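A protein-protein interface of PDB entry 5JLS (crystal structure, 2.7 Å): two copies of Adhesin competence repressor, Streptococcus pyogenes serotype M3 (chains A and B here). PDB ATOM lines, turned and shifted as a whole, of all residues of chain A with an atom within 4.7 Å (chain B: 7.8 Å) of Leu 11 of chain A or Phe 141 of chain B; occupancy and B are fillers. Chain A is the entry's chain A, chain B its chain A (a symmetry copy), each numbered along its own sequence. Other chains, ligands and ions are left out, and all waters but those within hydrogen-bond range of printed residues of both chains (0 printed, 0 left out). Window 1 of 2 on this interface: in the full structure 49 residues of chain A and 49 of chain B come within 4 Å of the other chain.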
ATOM      1  N   LYS A   7     -13.087 -11.396 -16.419  1.00  0.00           N
ATOM      2  CA  LYS A   7     -14.158 -12.381 -16.256  1.00  0.00           C
ATOM      3  C   LYS A   7     -14.048 -13.502 -17.293  1.00  0.00           C
ATOM      4  O   LYS A   7     -14.296 -14.686 -16.974  1.00  0.00           O
ATOM      5  CB  LYS A   7     -15.546 -11.782 -16.337  1.00  0.00           C
ATOM      6  CG  LYS A   7     -15.801 -10.670 -15.349  1.00  0.00           C
ATOM      7  CD  LYS A   7     -17.284 -10.537 -15.085  1.00  0.00           C
ATOM      8  CE  LYS A   7     -17.547  -9.760 -13.811  1.00  0.00           C
ATOM      9  NZ  LYS A   7     -19.018  -9.637 -13.590  1.00  0.00           N
ATOM     10  N   LEU A   8     -13.665 -13.125 -18.512  1.00  0.00           N
ATOM     11  CA  LEU A   8     -13.546 -14.090 -19.585  1.00  0.00           C
ATOM     12  C   LEU A   8     -12.408 -15.019 -19.345  1.00  0.00           C
ATOM     13  O   LEU A   8     -12.564 -16.245 -19.447  1.00  0.00           O
ATOM     14  CB  LEU A   8     -13.458 -13.422 -20.968  1.00  0.00           C
ATOM     15  CG  LEU A   8     -14.842 -13.146 -21.606  1.00  0.00           C
ATOM     16  CD1 LEU A   8     -14.688 -12.478 -22.961  1.00  0.00           C
ATOM     17  CD2 LEU A   8     -15.612 -14.455 -21.758  1.00  0.00           C
ATOM     18  N   ASP A   9     -11.278 -14.455 -18.944  1.00  0.00           N
ATOM     19  CA  ASP A   9     -10.096 -15.238 -18.775  1.00  0.00           C
ATOM     20  C   ASP A   9     -10.301 -16.257 -17.641  1.00  0.00           C
ATOM     21  O   ASP A   9      -9.795 -17.359 -17.721  1.00  0.00           O
ATOM     22  CB  ASP A   9      -8.939 -14.347 -18.447  1.00  0.00           C
ATOM     23  CG  ASP A   9      -7.615 -15.086 -18.452  1.00  0.00           C
ATOM     24  OD1 ASP A   9      -7.202 -15.667 -19.498  1.00  0.00           O
ATOM     25  OD2 ASP A   9      -6.983 -15.061 -17.390  1.00  0.00           O
ATOM     26  N   ASN A  10     -11.043 -15.869 -16.598  1.00  0.00           N
ATOM     27  CA  ASN A  10     -11.429 -16.769 -15.563  1.00  0.00           C
ATOM     28  C   ASN A  10     -12.329 -17.870 -16.022  1.00  0.00           C
ATOM     29  O   ASN A  10     -12.094 -19.022 -15.675  1.00  0.00           O
ATOM     30  CB  ASN A  10     -12.116 -16.031 -14.419  1.00  0.00           C
ATOM     31  CG  ASN A  10     -11.207 -15.004 -13.773  1.00  0.00           C
ATOM     32  OD1 ASN A  10     -10.087 -14.747 -14.235  1.00  0.00           O
ATOM     33  ND2 ASN A  10     -11.700 -14.379 -12.713  1.00  0.00           N
ATOM     34  N   LEU A  11     -13.377 -17.500 -16.746  1.00  0.00           N
ATOM     35  CA  LEU A  11     -14.346 -18.449 -17.232  1.00  0.00           C
ATOM     36  C   LEU A  11     -13.629 -19.610 -17.966  1.00  0.00           C
ATOM     37  O   LEU A  11     -13.916 -20.780 -17.761  1.00  0.00           O
ATOM     38  CB  LEU A  11     -15.378 -17.741 -18.119  1.00  0.00           C
ATOM     39  CG  LEU A  11     -16.370 -18.636 -18.878  1.00  0.00           C
ATOM     40  CD1 LEU A  11     -17.354 -19.238 -17.924  1.00  0.00           C
ATOM     41  CD2 LEU A  11     -17.147 -17.865 -19.927  1.00  0.00           C
ATOM     42  N   VAL A  12     -12.644 -19.259 -18.760  1.00  0.00           N
ATOM     43  CA  VAL A  12     -11.955 -20.205 -19.578  1.00  0.00           C
ATOM     44  C   VAL A  12     -11.064 -21.066 -18.671  1.00  0.00           C
ATOM     45  O   VAL A  12     -11.021 -22.322 -18.769  1.00  0.00           O
ATOM     46  CB  VAL A  12     -11.123 -19.463 -20.679  1.00  0.00           C
ATOM     47  CG1 VAL A  12     -10.442 -20.442 -21.602  1.00  0.00           C
ATOM     48  CG2 VAL A  12     -11.983 -18.562 -21.553  1.00  0.00           C
ATOM     49  N   ASN A  13     -10.336 -20.374 -17.812  1.00  0.00           N
ATOM     50  CA  ASN A  13      -9.497 -20.997 -16.807  1.00  0.00           C
ATOM     51  C   ASN A  13     -10.237 -22.035 -15.989  1.00  0.00           C
ATOM     52  O   ASN A  13      -9.674 -23.076 -15.699  1.00  0.00           O
ATOM     53  CB  ASN A  13      -8.886 -19.951 -15.865  1.00  0.00           C
ATOM     54  CG  ASN A  13      -7.726 -19.226 -16.472  1.00  0.00           C
ATOM     55  OD1 ASN A  13      -7.232 -19.596 -17.538  1.00  0.00           O
ATOM     56  ND2 ASN A  13      -7.279 -18.161 -15.799  1.00  0.00           N
ATOM     57  N   THR A  14     -11.493 -21.776 -15.639  1.00  0.00           N
ATOM     58  CA  THR A  14     -12.244 -22.764 -14.900  1.00  0.00           C
ATOM     59  C   THR A  14     -12.614 -23.873 -15.835  1.00  0.00           C
ATOM     60  O   THR A  14     -12.456 -25.050 -15.514  1.00  0.00           O
ATOM     61  CB  THR A  14     -13.478 -22.215 -14.165  1.00  0.00           C
ATOM     62  OG1 THR A  14     -14.556 -21.991 -15.083  1.00  0.00           O
ATOM     63  CG2 THR A  14     -13.102 -20.949 -13.375  1.00  0.00           C
ATOM     64  N   ILE A  15     -13.042 -23.527 -17.030  1.00  0.00           N
ATOM     65  CA  ILE A  15     -13.305 -24.581 -17.950  1.00  0.00           C
ATOM     66  C   ILE A  15     -12.096 -25.528 -18.031  1.00  0.00           C
ATOM     67  O   ILE A  15     -12.276 -26.735 -18.014  1.00  0.00           O
ATOM     68  CB  ILE A  15     -13.747 -24.047 -19.302  1.00  0.00           C
ATOM     69  CG1 ILE A  15     -15.152 -23.447 -19.172  1.00  0.00           C
ATOM     70  CG2 ILE A  15     -13.737 -25.178 -20.340  1.00  0.00           C
ATOM     71  CD1 ILE A  15     -15.494 -22.452 -20.258  1.00  0.00           C
ATOM     72  N   TYR A 119     -26.993 -25.894 -19.782  1.00  0.00           N
ATOM     73  CA  TYR A 119     -26.916 -24.744 -20.669  1.00  0.00           C
ATOM     74  C   TYR A 119     -28.303 -24.164 -20.906  1.00  0.00           C
ATOM     75  O   TYR A 119     -28.464 -22.974 -20.788  1.00  0.00           O
ATOM     76  CB  TYR A 119     -26.202 -25.050 -21.997  1.00  0.00           C
ATOM     77  CG  TYR A 119     -24.778 -25.484 -21.840  1.00  0.00           C
ATOM     78  CD1 TYR A 119     -23.965 -24.969 -20.830  1.00  0.00           C
ATOM     79  CD2 TYR A 119     -24.228 -26.404 -22.714  1.00  0.00           C
ATOM     80  CE1 TYR A 119     -22.654 -25.394 -20.677  1.00  0.00           C
ATOM     81  CE2 TYR A 119     -22.918 -26.843 -22.568  1.00  0.00           C
ATOM     82  CZ  TYR A 119     -22.125 -26.318 -21.555  1.00  0.00           C
ATOM     83  OH  TYR A 119     -20.805 -26.703 -21.416  1.00  0.00           O
ATOM     84  N   LEU A 122     -29.577 -22.347 -17.834  1.00  0.00           N
ATOM     85  CA  LEU A 122     -28.793 -21.153 -17.661  1.00  0.00           C
ATOM     86  C   LEU A 122     -29.296 -20.012 -18.595  1.00  0.00           C
ATOM     87  O   LEU A 122     -29.337 -18.815 -18.229  1.00  0.00           O
ATOM     88  CB  LEU A 122     -27.350 -21.553 -17.926  1.00  0.00           C
ATOM     89  CG  LEU A 122     -26.127 -20.657 -17.869  1.00  0.00           C
ATOM     90  CD1 LEU A 122     -24.927 -21.571 -18.071  1.00  0.00           C
ATOM     91  CD2 LEU A 122     -26.136 -19.564 -18.938  1.00  0.00           C
ATOM     92  N   LYS B   7     -24.392 -24.153 -29.331  1.00  0.00           N
ATOM     93  CA  LYS B   7     -23.288 -23.204 -29.486  1.00  0.00           C
ATOM     94  C   LYS B   7     -22.392 -23.182 -28.246  1.00  0.00           C
ATOM     95  O   LYS B   7     -21.150 -23.082 -28.364  1.00  0.00           O
ATOM     96  CB  LYS B   7     -23.744 -21.791 -29.779  1.00  0.00           C
ATOM     97  CG  LYS B   7     -24.624 -21.663 -30.998  1.00  0.00           C
ATOM     98  CD  LYS B   7     -24.552 -20.256 -31.549  1.00  0.00           C
ATOM     99  CE  LYS B   7     -25.053 -20.200 -32.978  1.00  0.00           C
ATOM    100  NZ  LYS B   7     -24.980 -18.797 -33.482  1.00  0.00           N
ATOM    101  N   LEU B   8     -23.021 -23.289 -27.077  1.00  0.00           N
ATOM    102  CA  LEU B   8     -22.286 -23.258 -25.830  1.00  0.00           C
ATOM    103  C   LEU B   8     -21.451 -24.481 -25.670  1.00  0.00           C
ATOM    104  O   LEU B   8     -20.256 -24.390 -25.357  1.00  0.00           O
ATOM    105  CB  LEU B   8     -23.199 -23.025 -24.615  1.00  0.00           C
ATOM    106  CG  LEU B   8     -23.440 -21.526 -24.307  1.00  0.00           C
ATOM    107  CD1 LEU B   8     -24.356 -21.363 -23.106  1.00  0.00           C
ATOM    108  CD2 LEU B   8     -22.108 -20.831 -24.040  1.00  0.00           C
ATOM    109  N   ASP B   9     -22.048 -25.627 -25.963  1.00  0.00           N
ATOM    110  CA  ASP B   9     -21.374 -26.869 -25.756  1.00  0.00           C
ATOM    111  C   ASP B   9     -20.151 -26.962 -26.683  1.00  0.00           C
ATOM    112  O   ASP B   9     -19.140 -27.515 -26.296  1.00  0.00           O
ATOM    113  CB  ASP B   9     -22.307 -28.006 -26.038  1.00  0.00           C
ATOM    114  CG  ASP B   9     -21.723 -29.349 -25.646  1.00  0.00           C
ATOM    115  OD1 ASP B   9     -21.388 -29.585 -24.448  1.00  0.00           O
ATOM    116  OD2 ASP B   9     -21.620 -30.176 -26.558  1.00  0.00           O
ATOM    117  N   LEU B  11     -18.453 -24.215 -27.857  1.00  0.00           N
ATOM    118  CA  LEU B  11     -17.512 -23.236 -27.377  1.00  0.00           C
ATOM    119  C   LEU B  11     -16.585 -23.869 -26.310  1.00  0.00           C
ATOM    120  O   LEU B  11     -15.374 -23.707 -26.327  1.00  0.00           O
ATOM    121  CB  LEU B  11     -18.258 -22.003 -26.851  1.00  0.00           C
ATOM    122  CG  LEU B  11     -17.418 -20.942 -26.123  1.00  0.00           C
ATOM    123  CD1 LEU B  11     -16.553 -20.210 -27.101  1.00  0.00           C
ATOM    124  CD2 LEU B  11     -18.281 -19.922 -25.407  1.00  0.00           C
ATOM    125  N   VAL B  12     -17.175 -24.651 -25.435  1.00  0.00           N
ATOM    126  CA  VAL B  12     -16.470 -25.225 -24.335  1.00  0.00           C
ATOM    127  C   VAL B  12     -15.556 -26.334 -24.876  1.00  0.00           C
ATOM    128  O   VAL B  12     -14.351 -26.442 -24.524  1.00  0.00           O
ATOM    129  CB  VAL B  12     -17.482 -25.771 -23.270  1.00  0.00           C
ATOM    130  CG1 VAL B  12     -16.764 -26.320 -22.063  1.00  0.00           C
ATOM    131  CG2 VAL B  12     -18.433 -24.696 -22.764  1.00  0.00           C
ATOM    132  N   ILE B  15     -12.646 -24.892 -26.327  1.00  0.00           N
ATOM    133  CA  ILE B  15     -11.755 -24.523 -25.280  1.00  0.00           C
ATOM    134  C   ILE B  15     -10.970 -25.753 -24.795  1.00  0.00           C
ATOM    135  O   ILE B  15      -9.767 -25.661 -24.604  1.00  0.00           O
ATOM    136  CB  ILE B  15     -12.477 -23.786 -24.164  1.00  0.00           C
ATOM    137  CG1 ILE B  15     -12.893 -22.398 -24.663  1.00  0.00           C
ATOM    138  CG2 ILE B  15     -11.561 -23.667 -22.938  1.00  0.00           C
ATOM    139  CD1 ILE B  15     -14.028 -21.782 -23.877  1.00  0.00           C
ATOM    140  N   TYR B 119      -9.379 -10.863 -25.743  1.00  0.00           N
ATOM    141  CA  TYR B 119     -10.673 -10.685 -25.103  1.00  0.00           C
ATOM    142  C   TYR B 119     -11.138  -9.244 -25.242  1.00  0.00           C
ATOM    143  O   TYR B 119     -12.264  -9.029 -25.621  1.00  0.00           O
ATOM    144  CB  TYR B 119     -10.689 -11.141 -23.633  1.00  0.00           C
ATOM    145  CG  TYR B 119     -10.384 -12.593 -23.439  1.00  0.00           C
ATOM    146  CD1 TYR B 119     -10.789 -13.555 -24.366  1.00  0.00           C
ATOM    147  CD2 TYR B 119      -9.701 -13.020 -22.315  1.00  0.00           C
ATOM    148  CE1 TYR B 119     -10.482 -14.895 -24.192  1.00  0.00           C
ATOM    149  CE2 TYR B 119      -9.381 -14.359 -22.131  1.00  0.00           C
ATOM    150  CZ  TYR B 119      -9.793 -15.301 -23.066  1.00  0.00           C
ATOM    151  OH  TYR B 119      -9.529 -16.645 -22.884  1.00  0.00           O
ATOM    152  N   VAL B 134     -23.583  -9.239 -21.709  1.00  0.00           N
ATOM    153  CA  VAL B 134     -22.457 -10.115 -21.850  1.00  0.00           C
ATOM    154  C   VAL B 134     -21.948 -10.429 -20.470  1.00  0.00           C
ATOM    155  O   VAL B 134     -21.780 -11.586 -20.158  1.00  0.00           O
ATOM    156  CB  VAL B 134     -21.388  -9.512 -22.795  1.00  0.00           C
ATOM    157  CG1 VAL B 134     -20.043 -10.219 -22.668  1.00  0.00           C
ATOM    158  CG2 VAL B 134     -21.900  -9.608 -24.226  1.00  0.00           C
ATOM    159  N   ASP B 135     -21.736  -9.376 -19.688  1.00  0.00           N
ATOM    160  CA  ASP B 135     -21.310  -9.415 -18.269  1.00  0.00           C
ATOM    161  C   ASP B 135     -22.216 -10.327 -17.460  1.00  0.00           C
ATOM    162  O   ASP B 135     -21.705 -11.251 -16.828  1.00  0.00           O
ATOM    163  CB  ASP B 135     -21.369  -7.990 -17.710  1.00  0.00           C
ATOM    164  CG  ASP B 135     -20.875  -7.864 -16.306  1.00  0.00           C
ATOM    165  OD1 ASP B 135     -20.605  -8.860 -15.638  1.00  0.00           O
ATOM    166  OD2 ASP B 135     -20.761  -6.712 -15.854  1.00  0.00           O
ATOM    167  N   LYS B 136     -23.533 -10.062 -17.518  1.00  0.00           N
ATOM    168  CA  LYS B 136     -24.558 -10.884 -16.901  1.00  0.00           C
ATOM    169  C   LYS B 136     -24.384 -12.362 -17.286  1.00  0.00           C
ATOM    170  O   LYS B 136     -24.140 -13.222 -16.416  1.00  0.00           O
ATOM    171  CB  LYS B 136     -25.961 -10.377 -17.298  1.00  0.00           C
ATOM    172  CG  LYS B 136     -27.162 -11.004 -16.555  1.00  0.00           C
ATOM    173  CD  LYS B 136     -28.515 -10.299 -16.876  1.00  0.00           C
ATOM    174  CE  LYS B 136     -29.766 -11.165 -16.608  1.00  0.00           C
ATOM    175  NZ  LYS B 136     -31.005 -10.685 -17.298  1.00  0.00           N
ATOM    176  N   PHE B 137     -24.461 -12.629 -18.589  1.00  0.00           N
ATOM    177  CA  PHE B 137     -24.212 -13.948 -19.154  1.00  0.00           C
ATOM    178  C   PHE B 137     -22.907 -14.634 -18.698  1.00  0.00           C
ATOM    179  O   PHE B 137     -22.909 -15.753 -18.178  1.00  0.00           O
ATOM    180  CB  PHE B 137     -24.241 -13.890 -20.694  1.00  0.00           C
ATOM    181  CG  PHE B 137     -23.828 -15.186 -21.319  1.00  0.00           C
ATOM    182  CD1 PHE B 137     -24.636 -16.308 -21.166  1.00  0.00           C
ATOM    183  CD2 PHE B 137     -22.591 -15.314 -21.940  1.00  0.00           C
ATOM    184  CE1 PHE B 137     -24.251 -17.512 -21.687  1.00  0.00           C
ATOM    185  CE2 PHE B 137     -22.191 -16.532 -22.440  1.00  0.00           C
ATOM    186  CZ  PHE B 137     -23.017 -17.633 -22.298  1.00  0.00           C
ATOM    187  N   VAL B 138     -21.776 -13.990 -18.872  1.00  0.00           N
ATOM    188  CA  VAL B 138     -20.540 -14.692 -18.511  1.00  0.00           C
ATOM    189  C   VAL B 138     -20.517 -14.888 -17.024  1.00  0.00           C
ATOM    190  O   VAL B 138     -19.818 -15.790 -16.561  1.00  0.00           O
ATOM    191  CB  VAL B 138     -19.192 -14.066 -19.011  1.00  0.00           C
ATOM    192  CG1 VAL B 138     -19.270 -13.638 -20.480  1.00  0.00           C
ATOM    193  CG2 VAL B 138     -18.722 -12.933 -18.123  1.00  0.00           C
ATOM    194  N   THR B 139     -21.266 -14.060 -16.285  1.00  0.00           N
ATOM    195  CA  THR B 139     -21.349 -14.190 -14.817  1.00  0.00           C
ATOM    196  C   THR B 139     -22.163 -15.409 -14.293  1.00  0.00           C
ATOM    197  O   THR B 139     -21.730 -16.090 -13.340  1.00  0.00           O
ATOM    198  CB  THR B 139     -21.834 -12.886 -14.175  1.00  0.00           C
ATOM    199  OG1 THR B 139     -20.986 -11.809 -14.595  1.00  0.00           O
ATOM    200  CG2 THR B 139     -21.757 -12.985 -12.683  1.00  0.00           C
ATOM    201  N   VAL B 140     -23.309 -15.693 -14.913  1.00  0.00           N
ATOM    202  CA  VAL B 140     -24.113 -16.860 -14.528  1.00  0.00           C
ATOM    203  C   VAL B 140     -23.441 -18.157 -15.056  1.00  0.00           C
ATOM    204  O   VAL B 140     -23.480 -19.249 -14.438  1.00  0.00           O
ATOM    205  CB  VAL B 140     -25.601 -16.707 -14.982  1.00  0.00           C
ATOM    206  CG1 VAL B 140     -26.135 -15.301 -14.672  1.00  0.00           C
ATOM    207  CG2 VAL B 140     -25.815 -17.014 -16.460  1.00  0.00           C
ATOM    208  N   PHE B 141     -22.808 -18.007 -16.213  1.00  0.00           N
ATOM    209  CA  PHE B 141     -22.065 -19.072 -16.801  1.00  0.00           C
ATOM    210  C   PHE B 141     -20.888 -19.349 -15.922  1.00  0.00           C
ATOM    211  O   PHE B 141     -20.592 -20.495 -15.671  1.00  0.00           O
ATOM    212  CB  PHE B 141     -21.610 -18.686 -18.202  1.00  0.00           C
ATOM    213  CG  PHE B 141     -21.214 -19.831 -19.059  1.00  0.00           C
ATOM    214  CD1 PHE B 141     -21.441 -21.160 -18.695  1.00  0.00           C
ATOM    215  CD2 PHE B 141     -20.640 -19.578 -20.278  1.00  0.00           C
ATOM    216  CE1 PHE B 141     -21.091 -22.198 -19.536  1.00  0.00           C
ATOM    217  CE2 PHE B 141     -20.274 -20.609 -21.117  1.00  0.00           C
ATOM    218  CZ  PHE B 141     -20.499 -21.919 -20.746  1.00  0.00           C
ATOM    219  N   ALA B 142     -20.260 -18.280 -15.432  1.00  0.00           N
ATOM    220  CA  ALA B 142     -19.160 -18.350 -14.459  1.00  0.00           C
ATOM    221  C   ALA B 142     -19.318 -19.524 -13.538  1.00  0.00           C
ATOM    222  O   ALA B 142     -18.628 -20.514 -13.724  1.00  0.00           O
ATOM    223  CB  ALA B 142     -19.021 -17.064 -13.644  1.00  0.00           C
ATOM    224  N   GLU B 143     -20.221 -19.473 -12.566  1.00  0.00           N
ATOM    225  CA  GLU B 143     -20.358 -20.651 -11.741  1.00  0.00           C
ATOM    226  C   GLU B 143     -21.752 -21.176 -11.834  1.00  0.00           C
ATOM    227  O   GLU B 143     -22.473 -21.139 -10.905  1.00  0.00           O
ATOM    228  CB  GLU B 143     -19.855 -20.442 -10.293  1.00  0.00           C
ATOM    229  CG  GLU B 143     -18.320 -20.370 -10.120  1.00  0.00           C
ATOM    230  CD  GLU B 143     -17.540 -21.646 -10.491  1.00  0.00           C
ATOM    231  OE1 GLU B 143     -18.095 -22.782 -10.457  1.00  0.00           O
ATOM    232  OE2 GLU B 143     -16.337 -21.497 -10.822  1.00  0.00           O
ATOM    233  N   GLU B 144     -22.141 -21.544 -13.031  1.00  0.00           N
ATOM    234  CA  GLU B 144     -22.956 -22.694 -13.256  1.00  0.00           C
ATOM    235  C   GLU B 144     -21.996 -23.826 -13.663  1.00  0.00           C
ATOM    236  O   GLU B 144     -22.388 -24.966 -13.777  1.00  0.00           O
ATOM    237  CB  GLU B 144     -23.981 -22.393 -14.349  1.00  0.00           C
ATOM    238  CG  GLU B 144     -25.009 -23.482 -14.581  1.00  0.00           C
ATOM    239  CD  GLU B 144     -25.820 -23.787 -13.337  1.00  0.00           C
ATOM    240  OE1 GLU B 144     -25.851 -24.962 -12.894  1.00  0.00           O
ATOM    241  OE2 GLU B 144     -26.410 -22.833 -12.791  1.00  0.00           O
ATOM    242  N   LEU B 145     -20.725 -23.504 -13.879  1.00  0.00           N
ATOM    243  CA  LEU B 145     -19.682 -24.508 -14.120  1.00  0.00           C
ATOM    244  C   LEU B 145     -19.171 -25.270 -12.905  1.00  0.00           C
ATOM    245  O   LEU B 145     -18.238 -26.069 -13.034  1.00  0.00           O
ATOM    246  CB  LEU B 145     -18.465 -23.852 -14.758  1.00  0.00           C
ATOM    247  CG  LEU B 145     -18.673 -23.321 -16.166  1.00  0.00           C
ATOM    248  CD1 LEU B 145     -17.361 -22.679 -16.579  1.00  0.00           C
ATOM    249  CD2 LEU B 145     -19.130 -24.403 -17.145  1.00  0.00           C
ATOM    250  N   GLU B 146     -19.740 -25.041 -11.731  1.00  0.00           N
ATOM    251  CA  GLU B 146     -19.361 -25.848 -10.576  1.00  0.00           C
ATOM    252  C   GLU B 146     -19.779 -27.345 -10.726  1.00  0.00           C
ATOM    253  O   GLU B 146     -18.961 -28.243 -10.500  1.00  0.00           O
ATOM    254  CB  GLU B 146     -19.924 -25.230  -9.295  1.00  0.00           C
ATOM    255  CG  GLU B 146     -18.993 -25.359  -8.106  1.00  0.00           C
ATOM    256  CD  GLU B 146     -19.331 -24.363  -7.031  1.00  0.00           C
ATOM    257  OE1 GLU B 146     -19.291 -23.151  -7.334  1.00  0.00           O
ATOM    258  OE2 GLU B 146     -19.635 -24.791  -5.899  1.00  0.00           O
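The side-chain amino group (NZ) of Lys 7 of chain A is in salt-bridge range of the side-chain carboxylate (OD1) of Asp 135 of chain B, at 2.7 Å. OG1 of Thr 139 of chain B lies within hydrogen-bond range of NZ of Lys 7 of chain A, 3.1 Å away.
ND2 of Asn 13 of chain A lies close to O of Asp 9 of chain A. The backbone carbonyl oxygen (O) of Asp 135 of chain B is in hydrogen-bond range of the side-chain hydroxyl (OG1) of Thr 139 of chain B, 2.4 Å away. OG1 of Thr 14 of chain A lies within hydrogen-bond range of O of Leu 11 of chain A (3.0 Å).
Among the printed residues, pairs that only touch across the chains: Thr 14 of chain A with Leu 145 of chain B (3.3 Å), Val 12 of chain A with Tyr 119 of chain B (3.4 Å), Tyr 119 of chain A with Val 12 of chain B (3.4 Å), Ile 15 of chain A with Leu 145 of chain B (3.5 Å), Asp 9 of chain A with Tyr 119 of chain B (3.5 Å), Tyr 119 of chain A with Asp 9 of chain B (3.5 Å), Leu 122 of chain A with Phe 141 of chain B (3.6 Å), Leu 122 of chain A with Val 140 of chain B (3.6 Å), Ile 15 of chain A with Val 12 of chain B (3.7 Å), Val 12 of chain A with Ile 15 of chain B (3.7 Å), Leu 11 of chain A with Leu 145 of chain B (3.7 Å), Ile 15 of chain A with Ile 15 of chain B (3.7 Å), Tyr 119 of chain A with Phe 141 of chain B (3.7 Å), Lys 7 of chain A with Val 138 of chain B (3.8 Å), Leu 11 of chain A with Phe 141 of chain B (3.9 Å), Leu 122 of chain A with Phe 137 of chain B (3.9 Å), Leu 122 of chain A with Glu 144 of chain B (3.9 Å), Leu 11 of chain A with Ala 142 of chain B (3.9 Å) and Leu 8 of chain A with Val 138 of chain B (3.96 Å).
Printed residues of chain B within 4 Å of Leu 11 of chain A: Phe 141, Ala 142 and Leu 145. Of the printed residues of chain A, Val 12 of chain B touches Ile 15 (3.7 Å) and Tyr 119 (3.4 Å). Of the printed residues of chain A, Tyr 119 of chain B touches Asp 9 and Val 12. Of chain A, only Leu 11, Tyr 119 and Leu 122 come within 4 Å of Phe 141 of chain B. Printed residues of chain A within 4 Å of Ala 142 of chain B: Leu 11. The nearest residue of chain B that does not touch Leu 11 of chain A is Val 138 of chain B (4.4 Å). The nearest printed residue of chain B that does not touch Leu 8 of chain A is Tyr 119 of chain B (4.01 Å).
Printed residues of chain B that touch a printed residue of chain A: Asp 9, Val 12, Ile 15, Tyr 119, Asp 135, Phe 137, Val 138, Thr 139, Val 140, Phe 141, Ala 142, Glu 144 and Leu 145. Hydrophobic or aromatic side chains of chain B that line the printed part of chain A: Val 12, Ile 15, Tyr 119, Phe 137, Val 138, Val 140, Phe 141 and Leu 145. Of the 11 printed residues of chain A, 9 touch a printed residue of chain B. Hydrophobic or aromatic side chains of chain A within 4 Å of the printed part of chain B: Leu 8, Leu 11, Val 12, Ile 15, Tyr 119 and Leu 122. Among the printed residues, Asp or Glu carboxylates within 4 Å of a Lys or Arg side-chain nitrogen of the other chain: Lys 7 of chain A with Asp 135 of chain B (2.7 Å).
Asp 9 of chain A touches Tyr 119 of chain B, and with the chains exchanged Tyr 119 of chain A touches Asp 9 of chain B. Val 12 of chain A touches Ile 15 of chain B, and with the chains exchanged Ile 15 of chain A touches Val 12 of chain B. Val 12 of chain A touches Tyr 119 of chain B, and with the chains exchanged Tyr 119 of chain A touches Val 12 of chain B. Ile 15 of chain A touches its own counterpart, Ile 15 of chain B.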
